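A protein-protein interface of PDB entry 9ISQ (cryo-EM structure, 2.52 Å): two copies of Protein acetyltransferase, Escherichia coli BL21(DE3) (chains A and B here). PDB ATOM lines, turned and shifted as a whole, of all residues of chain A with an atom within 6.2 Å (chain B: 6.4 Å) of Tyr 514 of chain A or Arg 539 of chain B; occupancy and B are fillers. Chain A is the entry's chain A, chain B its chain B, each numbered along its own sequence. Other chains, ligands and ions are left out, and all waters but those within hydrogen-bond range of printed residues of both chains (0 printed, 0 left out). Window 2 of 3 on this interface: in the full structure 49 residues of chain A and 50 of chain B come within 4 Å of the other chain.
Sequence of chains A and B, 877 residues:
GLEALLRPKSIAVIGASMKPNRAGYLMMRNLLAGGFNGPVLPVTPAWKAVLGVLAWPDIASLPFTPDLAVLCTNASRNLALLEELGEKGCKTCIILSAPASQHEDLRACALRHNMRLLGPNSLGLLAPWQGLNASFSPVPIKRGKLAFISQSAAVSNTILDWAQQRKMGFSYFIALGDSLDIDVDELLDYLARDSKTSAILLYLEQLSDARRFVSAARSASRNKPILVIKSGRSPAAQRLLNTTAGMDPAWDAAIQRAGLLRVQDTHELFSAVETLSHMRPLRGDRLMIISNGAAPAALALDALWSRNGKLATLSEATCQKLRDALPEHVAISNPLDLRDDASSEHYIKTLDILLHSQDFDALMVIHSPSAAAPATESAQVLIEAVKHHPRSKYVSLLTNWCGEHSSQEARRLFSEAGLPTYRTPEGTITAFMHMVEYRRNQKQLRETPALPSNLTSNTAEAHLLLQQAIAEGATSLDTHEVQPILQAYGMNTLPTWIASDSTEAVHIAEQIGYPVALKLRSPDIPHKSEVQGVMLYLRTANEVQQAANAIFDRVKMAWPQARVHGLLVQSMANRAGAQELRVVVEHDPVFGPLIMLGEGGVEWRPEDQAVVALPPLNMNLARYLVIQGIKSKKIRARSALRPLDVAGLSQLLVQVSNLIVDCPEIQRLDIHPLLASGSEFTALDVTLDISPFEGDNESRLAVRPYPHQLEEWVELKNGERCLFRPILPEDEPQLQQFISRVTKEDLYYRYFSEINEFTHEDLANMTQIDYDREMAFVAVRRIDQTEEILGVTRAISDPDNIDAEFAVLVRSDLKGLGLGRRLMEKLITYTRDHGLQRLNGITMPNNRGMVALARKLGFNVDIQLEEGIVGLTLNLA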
ATOM      1  N   ALA A 505     -16.101  14.268  12.072  1.00  0.00           N
ATOM      2  CA  ALA A 505     -14.893  15.068  12.222  1.00  0.00           C
ATOM      3  C   ALA A 505     -14.878  15.773  13.570  1.00  0.00           C
ATOM      4  O   ALA A 505     -13.913  15.659  14.332  1.00  0.00           O
ATOM      5  CB  ALA A 505     -14.790  16.081  11.082  1.00  0.00           C
ATOM      6  N   VAL A 506     -15.954  16.493  13.892  1.00  0.00           N
ATOM      7  CA  VAL A 506     -16.019  17.158  15.191  1.00  0.00           C
ATOM      8  C   VAL A 506     -16.143  16.141  16.317  1.00  0.00           C
ATOM      9  O   VAL A 506     -15.595  16.344  17.409  1.00  0.00           O
ATOM     10  CB  VAL A 506     -17.172  18.178  15.218  1.00  0.00           C
ATOM     11  CG1 VAL A 506     -16.923  19.267  14.198  1.00  0.00           C
ATOM     12  CG2 VAL A 506     -18.514  17.497  14.962  1.00  0.00           C
ATOM     13  N   ALA A 509     -12.698  15.296  16.915  1.00  0.00           N
ATOM     14  CA  ALA A 509     -11.893  16.450  17.299  1.00  0.00           C
ATOM     15  C   ALA A 509     -12.096  16.791  18.766  1.00  0.00           C
ATOM     16  O   ALA A 509     -11.133  17.095  19.481  1.00  0.00           O
ATOM     17  CB  ALA A 509     -12.241  17.647  16.416  1.00  0.00           C
ATOM     18  N   GLU A 510     -13.343  16.747  19.235  1.00  0.00           N
ATOM     19  CA  GLU A 510     -13.603  17.016  20.643  1.00  0.00           C
ATOM     20  C   GLU A 510     -12.897  16.011  21.540  1.00  0.00           C
ATOM     21  O   GLU A 510     -12.546  16.335  22.680  1.00  0.00           O
ATOM     22  CB  GLU A 510     -15.106  16.998  20.914  1.00  0.00           C
ATOM     23  CG  GLU A 510     -15.734  15.624  20.793  1.00  0.00           C
ATOM     24  CD  GLU A 510     -17.156  15.678  20.275  1.00  0.00           C
ATOM     25  OE1 GLU A 510     -17.403  16.398  19.286  1.00  0.00           O
ATOM     26  OE2 GLU A 510     -18.027  14.998  20.856  1.00  0.00           O
ATOM     27  N   ILE A 512      -9.870  14.147  20.698  1.00  0.00           N
ATOM     28  CA  ILE A 512      -8.421  14.325  20.656  1.00  0.00           C
ATOM     29  C   ILE A 512      -8.026  15.621  21.354  1.00  0.00           C
ATOM     30  O   ILE A 512      -6.995  15.687  22.034  1.00  0.00           O
ATOM     31  CB  ILE A 512      -7.912  14.278  19.203  1.00  0.00           C
ATOM     32  CG1 ILE A 512      -8.595  15.350  18.352  1.00  0.00           C
ATOM     33  CG2 ILE A 512      -8.146  12.895  18.611  1.00  0.00           C
ATOM     34  CD1 ILE A 512      -8.156  15.354  16.903  1.00  0.00           C
ATOM     35  N   GLY A 513      -8.831  16.668  21.197  1.00  0.00           N
ATOM     36  CA  GLY A 513      -8.586  17.922  21.881  1.00  0.00           C
ATOM     37  C   GLY A 513      -8.145  19.035  20.954  1.00  0.00           C
ATOM     38  O   GLY A 513      -7.172  18.886  20.209  1.00  0.00           O
ATOM     39  N   TYR A 514      -8.855  20.160  20.994  1.00  0.00           N
ATOM     40  CA  TYR A 514      -8.508  21.295  20.159  1.00  0.00           C
ATOM     41  C   TYR A 514      -7.194  21.914  20.630  1.00  0.00           C
ATOM     42  O   TYR A 514      -6.806  21.761  21.791  1.00  0.00           O
ATOM     43  CB  TYR A 514      -9.622  22.337  20.189  1.00  0.00           C
ATOM     44  CG  TYR A 514     -10.898  21.888  19.513  1.00  0.00           C
ATOM     45  CD1 TYR A 514     -11.096  22.092  18.154  1.00  0.00           C
ATOM     46  CD2 TYR A 514     -11.905  21.262  20.234  1.00  0.00           C
ATOM     47  CE1 TYR A 514     -12.260  21.684  17.533  1.00  0.00           C
ATOM     48  CE2 TYR A 514     -13.073  20.850  19.622  1.00  0.00           C
ATOM     49  CZ  TYR A 514     -13.245  21.063  18.271  1.00  0.00           C
ATOM     50  OH  TYR A 514     -14.406  20.655  17.657  1.00  0.00           O
ATOM     51  N   PRO A 515      -6.479  22.619  19.740  1.00  0.00           N
ATOM     52  CA  PRO A 515      -6.797  22.895  18.329  1.00  0.00           C
ATOM     53  C   PRO A 515      -6.680  21.646  17.465  1.00  0.00           C
ATOM     54  O   PRO A 515      -6.351  20.574  17.963  1.00  0.00           O
ATOM     55  CB  PRO A 515      -5.763  23.965  17.931  1.00  0.00           C
ATOM     56  CG  PRO A 515      -5.094  24.413  19.203  1.00  0.00           C
ATOM     57  CD  PRO A 515      -5.225  23.267  20.152  1.00  0.00           C
ATOM     58  N   VAL A 516      -6.950  21.754  16.168  1.00  0.00           N
ATOM     59  CA  VAL A 516      -6.983  20.590  15.292  1.00  0.00           C
ATOM     60  C   VAL A 516      -6.739  21.063  13.867  1.00  0.00           C
ATOM     61  O   VAL A 516      -7.224  22.124  13.463  1.00  0.00           O
ATOM     62  CB  VAL A 516      -8.332  19.840  15.430  1.00  0.00           C
ATOM     63  CG1 VAL A 516      -8.638  19.051  14.174  1.00  0.00           C
ATOM     64  CG2 VAL A 516      -8.321  18.938  16.659  1.00  0.00           C
ATOM     65  N   MET A 535      -6.063  25.028   9.979  1.00  0.00           N
ATOM     66  CA  MET A 535      -6.754  25.778  11.017  1.00  0.00           C
ATOM     67  C   MET A 535      -5.981  25.608  12.316  1.00  0.00           C
ATOM     68  O   MET A 535      -5.498  24.516  12.626  1.00  0.00           O
ATOM     69  CB  MET A 535      -8.211  25.293  11.161  1.00  0.00           C
ATOM     70  CG  MET A 535      -9.070  25.981  12.232  1.00  0.00           C
ATOM     71  SD  MET A 535      -8.497  25.866  13.941  1.00  0.00           S
ATOM     72  CE  MET A 535      -9.703  24.733  14.634  1.00  0.00           C
ATOM     73  N   LEU A 538      -7.878  27.788  17.427  1.00  0.00           N
ATOM     74  CA  LEU A 538      -9.322  27.861  17.635  1.00  0.00           C
ATOM     75  C   LEU A 538      -9.815  26.537  18.204  1.00  0.00           C
ATOM     76  O   LEU A 538      -9.172  25.500  18.010  1.00  0.00           O
ATOM     77  CB  LEU A 538     -10.059  28.174  16.328  1.00  0.00           C
ATOM     78  CG  LEU A 538     -11.583  28.031  16.302  1.00  0.00           C
ATOM     79  CD1 LEU A 538     -12.181  29.146  15.463  1.00  0.00           C
ATOM     80  CD2 LEU A 538     -12.015  26.680  15.767  1.00  0.00           C
ATOM     81  N   ARG A 539     -10.952  26.573  18.901  1.00  0.00           N
ATOM     82  CA  ARG A 539     -11.505  25.386  19.540  1.00  0.00           C
ATOM     83  C   ARG A 539     -13.002  25.207  19.320  1.00  0.00           C
ATOM     84  O   ARG A 539     -13.571  24.239  19.838  1.00  0.00           O
ATOM     85  CB  ARG A 539     -11.224  25.419  21.046  1.00  0.00           C
ATOM     86  CG  ARG A 539      -9.769  25.660  21.411  1.00  0.00           C
ATOM     87  CD  ARG A 539      -9.571  25.586  22.916  1.00  0.00           C
ATOM     88  NE  ARG A 539     -10.276  26.651  23.621  1.00  0.00           N
ATOM     89  CZ  ARG A 539     -10.551  26.636  24.918  1.00  0.00           C
ATOM     90  NH1 ARG A 539     -10.207  25.615  25.688  1.00  0.00           N
ATOM     91  NH2 ARG A 539     -11.190  27.669  25.459  1.00  0.00           N
ATOM     92  N   THR A 540     -13.661  26.095  18.579  1.00  0.00           N
ATOM     93  CA  THR A 540     -15.099  25.973  18.372  1.00  0.00           C
ATOM     94  C   THR A 540     -15.395  24.976  17.258  1.00  0.00           C
ATOM     95  O   THR A 540     -14.653  24.886  16.275  1.00  0.00           O
ATOM     96  CB  THR A 540     -15.723  27.332  18.045  1.00  0.00           C
ATOM     97  OG1 THR A 540     -17.148  27.194  17.965  1.00  0.00           O
ATOM     98  CG2 THR A 540     -15.190  27.898  16.732  1.00  0.00           C
ATOM     99  N   ALA A 541     -16.484  24.224  17.420  1.00  0.00           N
ATOM    100  CA  ALA A 541     -16.854  23.214  16.436  1.00  0.00           C
ATOM    101  C   ALA A 541     -17.490  23.830  15.194  1.00  0.00           C
ATOM    102  O   ALA A 541     -17.303  23.322  14.083  1.00  0.00           O
ATOM    103  CB  ALA A 541     -17.809  22.200  17.066  1.00  0.00           C
ATOM    104  N   ASN A 542     -18.248  24.917  15.363  1.00  0.00           N
ATOM    105  CA  ASN A 542     -18.969  25.494  14.233  1.00  0.00           C
ATOM    106  C   ASN A 542     -18.011  25.967  13.150  1.00  0.00           C
ATOM    107  O   ASN A 542     -18.315  25.868  11.955  1.00  0.00           O
ATOM    108  CB  ASN A 542     -19.853  26.648  14.704  1.00  0.00           C
ATOM    109  CG  ASN A 542     -20.612  27.299  13.565  1.00  0.00           C
ATOM    110  OD1 ASN A 542     -20.800  26.700  12.506  1.00  0.00           O
ATOM    111  ND2 ASN A 542     -21.053  28.533  13.777  1.00  0.00           N
ATOM    112  N   VAL A 544     -15.207  24.524  12.427  1.00  0.00           N
ATOM    113  CA  VAL A 544     -14.826  23.302  11.727  1.00  0.00           C
ATOM    114  C   VAL A 544     -15.922  22.888  10.755  1.00  0.00           C
ATOM    115  O   VAL A 544     -15.646  22.513   9.609  1.00  0.00           O
ATOM    116  CB  VAL A 544     -14.514  22.185  12.742  1.00  0.00           C
ATOM    117  CG1 VAL A 544     -14.344  20.849  12.031  1.00  0.00           C
ATOM    118  CG2 VAL A 544     -13.268  22.530  13.548  1.00  0.00           C
ATOM    119  N   MET A 572      -2.945  18.468  17.473  1.00  0.00           N
ATOM    120  CA  MET A 572      -1.756  19.296  17.594  1.00  0.00           C
ATOM    121  C   MET A 572      -1.073  19.032  18.927  1.00  0.00           C
ATOM    122  O   MET A 572      -1.735  18.784  19.940  1.00  0.00           O
ATOM    123  CB  MET A 572      -2.096  20.787  17.486  1.00  0.00           C
ATOM    124  CG  MET A 572      -3.383  21.094  16.745  1.00  0.00           C
ATOM    125  SD  MET A 572      -3.502  20.270  15.148  1.00  0.00           S
ATOM    126  CE  MET A 572      -1.912  20.679  14.432  1.00  0.00           C
ATOM    127  N   ALA A 573       0.256  19.076  18.913  1.00  0.00           N
ATOM    128  CA  ALA A 573       1.095  19.039  20.094  1.00  0.00           C
ATOM    129  C   ALA A 573       1.579  20.462  20.381  1.00  0.00           C
ATOM    130  O   ALA A 573       1.122  21.415  19.725  1.00  0.00           O
ATOM    131  CB  ALA A 573       2.219  18.032  19.873  1.00  0.00           C
ATOM    132  N   ASN A 574       2.486  20.612  21.346  1.00  0.00           N
ATOM    133  CA  ASN A 574       3.064  21.924  21.658  1.00  0.00           C
ATOM    134  C   ASN A 574       4.043  22.510  20.635  1.00  0.00           C
ATOM    135  O   ASN A 574       5.256  22.589  20.843  1.00  0.00           O
ATOM    136  CB  ASN A 574       3.137  22.340  23.125  1.00  0.00           C
ATOM    137  CG  ASN A 574       1.793  22.268  23.814  1.00  0.00           C
ATOM    138  OD1 ASN A 574       1.193  21.199  23.923  1.00  0.00           O
ATOM    139  ND2 ASN A 574       1.307  23.410  24.280  1.00  0.00           N
ATOM    140  N   TYR B 514      -8.310  29.351  26.447  1.00  0.00           N
ATOM    141  CA  TYR B 514      -7.011  28.823  26.080  1.00  0.00           C
ATOM    142  C   TYR B 514      -6.769  29.002  24.584  1.00  0.00           C
ATOM    143  O   TYR B 514      -7.715  29.123  23.802  1.00  0.00           O
ATOM    144  CB  TYR B 514      -6.913  27.347  26.454  1.00  0.00           C
ATOM    145  CG  TYR B 514      -7.018  27.080  27.939  1.00  0.00           C
ATOM    146  CD1 TYR B 514      -8.254  26.936  28.555  1.00  0.00           C
ATOM    147  CD2 TYR B 514      -5.879  26.974  28.725  1.00  0.00           C
ATOM    148  CE1 TYR B 514      -8.349  26.690  29.913  1.00  0.00           C
ATOM    149  CE2 TYR B 514      -5.964  26.728  30.079  1.00  0.00           C
ATOM    150  CZ  TYR B 514      -7.201  26.588  30.667  1.00  0.00           C
ATOM    151  OH  TYR B 514      -7.290  26.344  32.019  1.00  0.00           O
ATOM    152  N   PRO B 515      -5.500  29.028  24.158  1.00  0.00           N
ATOM    153  CA  PRO B 515      -4.271  28.919  24.960  1.00  0.00           C
ATOM    154  C   PRO B 515      -3.969  30.220  25.694  1.00  0.00           C
ATOM    155  O   PRO B 515      -4.660  31.215  25.497  1.00  0.00           O
ATOM    156  CB  PRO B 515      -3.192  28.577  23.917  1.00  0.00           C
ATOM    157  CG  PRO B 515      -3.914  28.337  22.610  1.00  0.00           C
ATOM    158  CD  PRO B 515      -5.198  29.090  22.722  1.00  0.00           C
ATOM    159  N   VAL B 516      -2.948  30.249  26.546  1.00  0.00           N
ATOM    160  CA  VAL B 516      -2.659  31.425  27.357  1.00  0.00           C
ATOM    161  C   VAL B 516      -1.150  31.562  27.509  1.00  0.00           C
ATOM    162  O   VAL B 516      -0.434  30.565  27.637  1.00  0.00           O
ATOM    163  CB  VAL B 516      -3.359  31.327  28.728  1.00  0.00           C
ATOM    164  CG1 VAL B 516      -2.773  32.330  29.698  1.00  0.00           C
ATOM    165  CG2 VAL B 516      -4.859  31.531  28.565  1.00  0.00           C
ATOM    166  N   TYR B 537       0.989  27.919  24.861  1.00  0.00           N
ATOM    167  CA  TYR B 537       0.100  27.070  24.078  1.00  0.00           C
ATOM    168  C   TYR B 537      -0.420  25.860  24.861  1.00  0.00           C
ATOM    169  O   TYR B 537      -1.257  25.126  24.332  1.00  0.00           O
ATOM    170  CB  TYR B 537       0.763  26.563  22.780  1.00  0.00           C
ATOM    171  CG  TYR B 537      -0.150  26.479  21.571  1.00  0.00           C
ATOM    172  CD1 TYR B 537      -1.521  26.296  21.707  1.00  0.00           C
ATOM    173  CD2 TYR B 537       0.368  26.587  20.287  1.00  0.00           C
ATOM    174  CE1 TYR B 537      -2.346  26.220  20.600  1.00  0.00           C
ATOM    175  CE2 TYR B 537      -0.449  26.514  19.175  1.00  0.00           C
ATOM    176  CZ  TYR B 537      -1.804  26.331  19.337  1.00  0.00           C
ATOM    177  OH  TYR B 537      -2.620  26.258  18.231  1.00  0.00           O
ATOM    178  N   LEU B 538       0.028  25.621  26.092  1.00  0.00           N
ATOM    179  CA  LEU B 538      -0.475  24.490  26.865  1.00  0.00           C
ATOM    180  C   LEU B 538      -1.840  24.843  27.442  1.00  0.00           C
ATOM    181  O   LEU B 538      -2.102  26.005  27.768  1.00  0.00           O
ATOM    182  CB  LEU B 538       0.505  24.108  27.971  1.00  0.00           C
ATOM    183  CG  LEU B 538       1.641  23.182  27.529  1.00  0.00           C
ATOM    184  CD1 LEU B 538       2.794  23.991  26.959  1.00  0.00           C
ATOM    185  CD2 LEU B 538       2.117  22.312  28.679  1.00  0.00           C
ATOM    186  N   ARG B 539      -2.708  23.838  27.566  1.00  0.00           N
ATOM    187  CA  ARG B 539      -4.109  24.041  27.913  1.00  0.00           C
ATOM    188  C   ARG B 539      -4.517  23.276  29.170  1.00  0.00           C
ATOM    189  O   ARG B 539      -5.596  22.682  29.217  1.00  0.00           O
ATOM    190  CB  ARG B 539      -4.992  23.643  26.733  1.00  0.00           C
ATOM    191  CG  ARG B 539      -4.733  24.463  25.480  1.00  0.00           C
ATOM    192  CD  ARG B 539      -4.399  23.582  24.290  1.00  0.00           C
ATOM    193  NE  ARG B 539      -3.077  22.979  24.421  1.00  0.00           N
ATOM    194  CZ  ARG B 539      -2.491  22.240  23.489  1.00  0.00           C
ATOM    195  NH1 ARG B 539      -3.081  21.989  22.332  1.00  0.00           N
ATOM    196  NH2 ARG B 539      -1.281  21.741  23.723  1.00  0.00           N
ATOM    197  N   THR B 540      -3.667  23.282  30.192  1.00  0.00           N
ATOM    198  CA  THR B 540      -3.963  22.646  31.469  1.00  0.00           C
ATOM    199  C   THR B 540      -3.655  23.615  32.601  1.00  0.00           C
ATOM    200  O   THR B 540      -2.573  24.210  32.639  1.00  0.00           O
ATOM    201  CB  THR B 540      -3.158  21.358  31.639  1.00  0.00           C
ATOM    202  OG1 THR B 540      -3.193  20.944  33.011  1.00  0.00           O
ATOM    203  CG2 THR B 540      -1.720  21.563  31.198  1.00  0.00           C
ATOM    204  N   ALA B 541      -4.607  23.766  33.525  1.00  0.00           N
ATOM    205  CA  ALA B 541      -4.435  24.721  34.614  1.00  0.00           C
ATOM    206  C   ALA B 541      -3.275  24.331  35.522  1.00  0.00           C
ATOM    207  O   ALA B 541      -2.470  25.185  35.910  1.00  0.00           O
ATOM    208  CB  ALA B 541      -5.727  24.832  35.420  1.00  0.00           C
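Tyr 514 of chain A touches Arg 539 of chain B, and with the chains exchanged Arg 539 of chain A touches Tyr 514 of chain B.
Pro 515 of chain A touches Arg 539 of chain B, but with the chains exchanged Arg 539 of chain A does not touch Pro 515 of chain B (5.4 Å).
Of the 7 pairs that touch across the chains among the printed residues, 2 have their exchanged pair printed and touching as well.
The backbone NH (N) of Tyr 514 of chain B lies close to the guanidinium group (NH2) of Arg 539 of chain A (3.5 Å).
The side-chain amide nitrogen of Asn 574 of chain A lies close to the backbone carbonyl oxygen of Tyr 537 of chain B, 3.1 Å away.
The side-chain amide nitrogen (ND2) of Asn 574 of chain A lies close to the backbone NH (N) of Leu 538 of chain B, 3.1 Å away.
The side-chain amide oxygen of Asn 574 of chain A is in hydrogen-bond range of the guanidinium group of Arg 539 of chain B (2.5 Å).
The guanidinium group (NE) of Arg 539 of chain B is in hydrogen-bond range of the backbone carbonyl oxygen (O) of Tyr 537 of chain B.
Among the printed residues, pairs that only touch across the chains: Tyr 514 of chain A with Arg 539 of chain B (3.8 Å), Pro 515 of chain A with Tyr 537 of chain B (3.2 Å) and Pro 515 of chain A with Arg 539 of chain B (3.3 Å).
Tyr 514 of chain A touches just one residue of chain B: Arg 539 (3.8 Å).
Of the printed residues of chain B, Pro 515 of chain A touches Tyr 537 (3.2 Å) and Arg 539 (3.3 Å).
Printed residues of chain B within 4 Å of Arg 539 of chain A: Tyr 514 (3.5 Å).
Of the printed residues of chain B, Asn 574 of chain A touches Tyr 537 (3.1 Å), Leu 538 (3.1 Å) and Arg 539 (2.5 Å).
Printed residues of chain A within 4 Å of Tyr 514 of chain B: Arg 539.
Arg 539 of chain B touches three residues of chain A.
The nearest printed residue of chain B that does not touch Asn 574 of chain A is Pro 515 of chain B (6.9 Å).
Of the 19 printed residues of chain A, 4 touch a printed residue of chain B.
Printed residues of chain A that touch a printed residue of chain B: Tyr 514, Pro 515, Arg 539 and Asn 574.
Along chain B the printed residues that touch a printed residue of chain A span positions 514 to 539.
Among the printed residues, 7 pairs touch across the chains.
Among the printed residues, no Asp or Glu carboxylate lies within 4 Å of a Lys or Arg side-chain nitrogen of the other chain.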
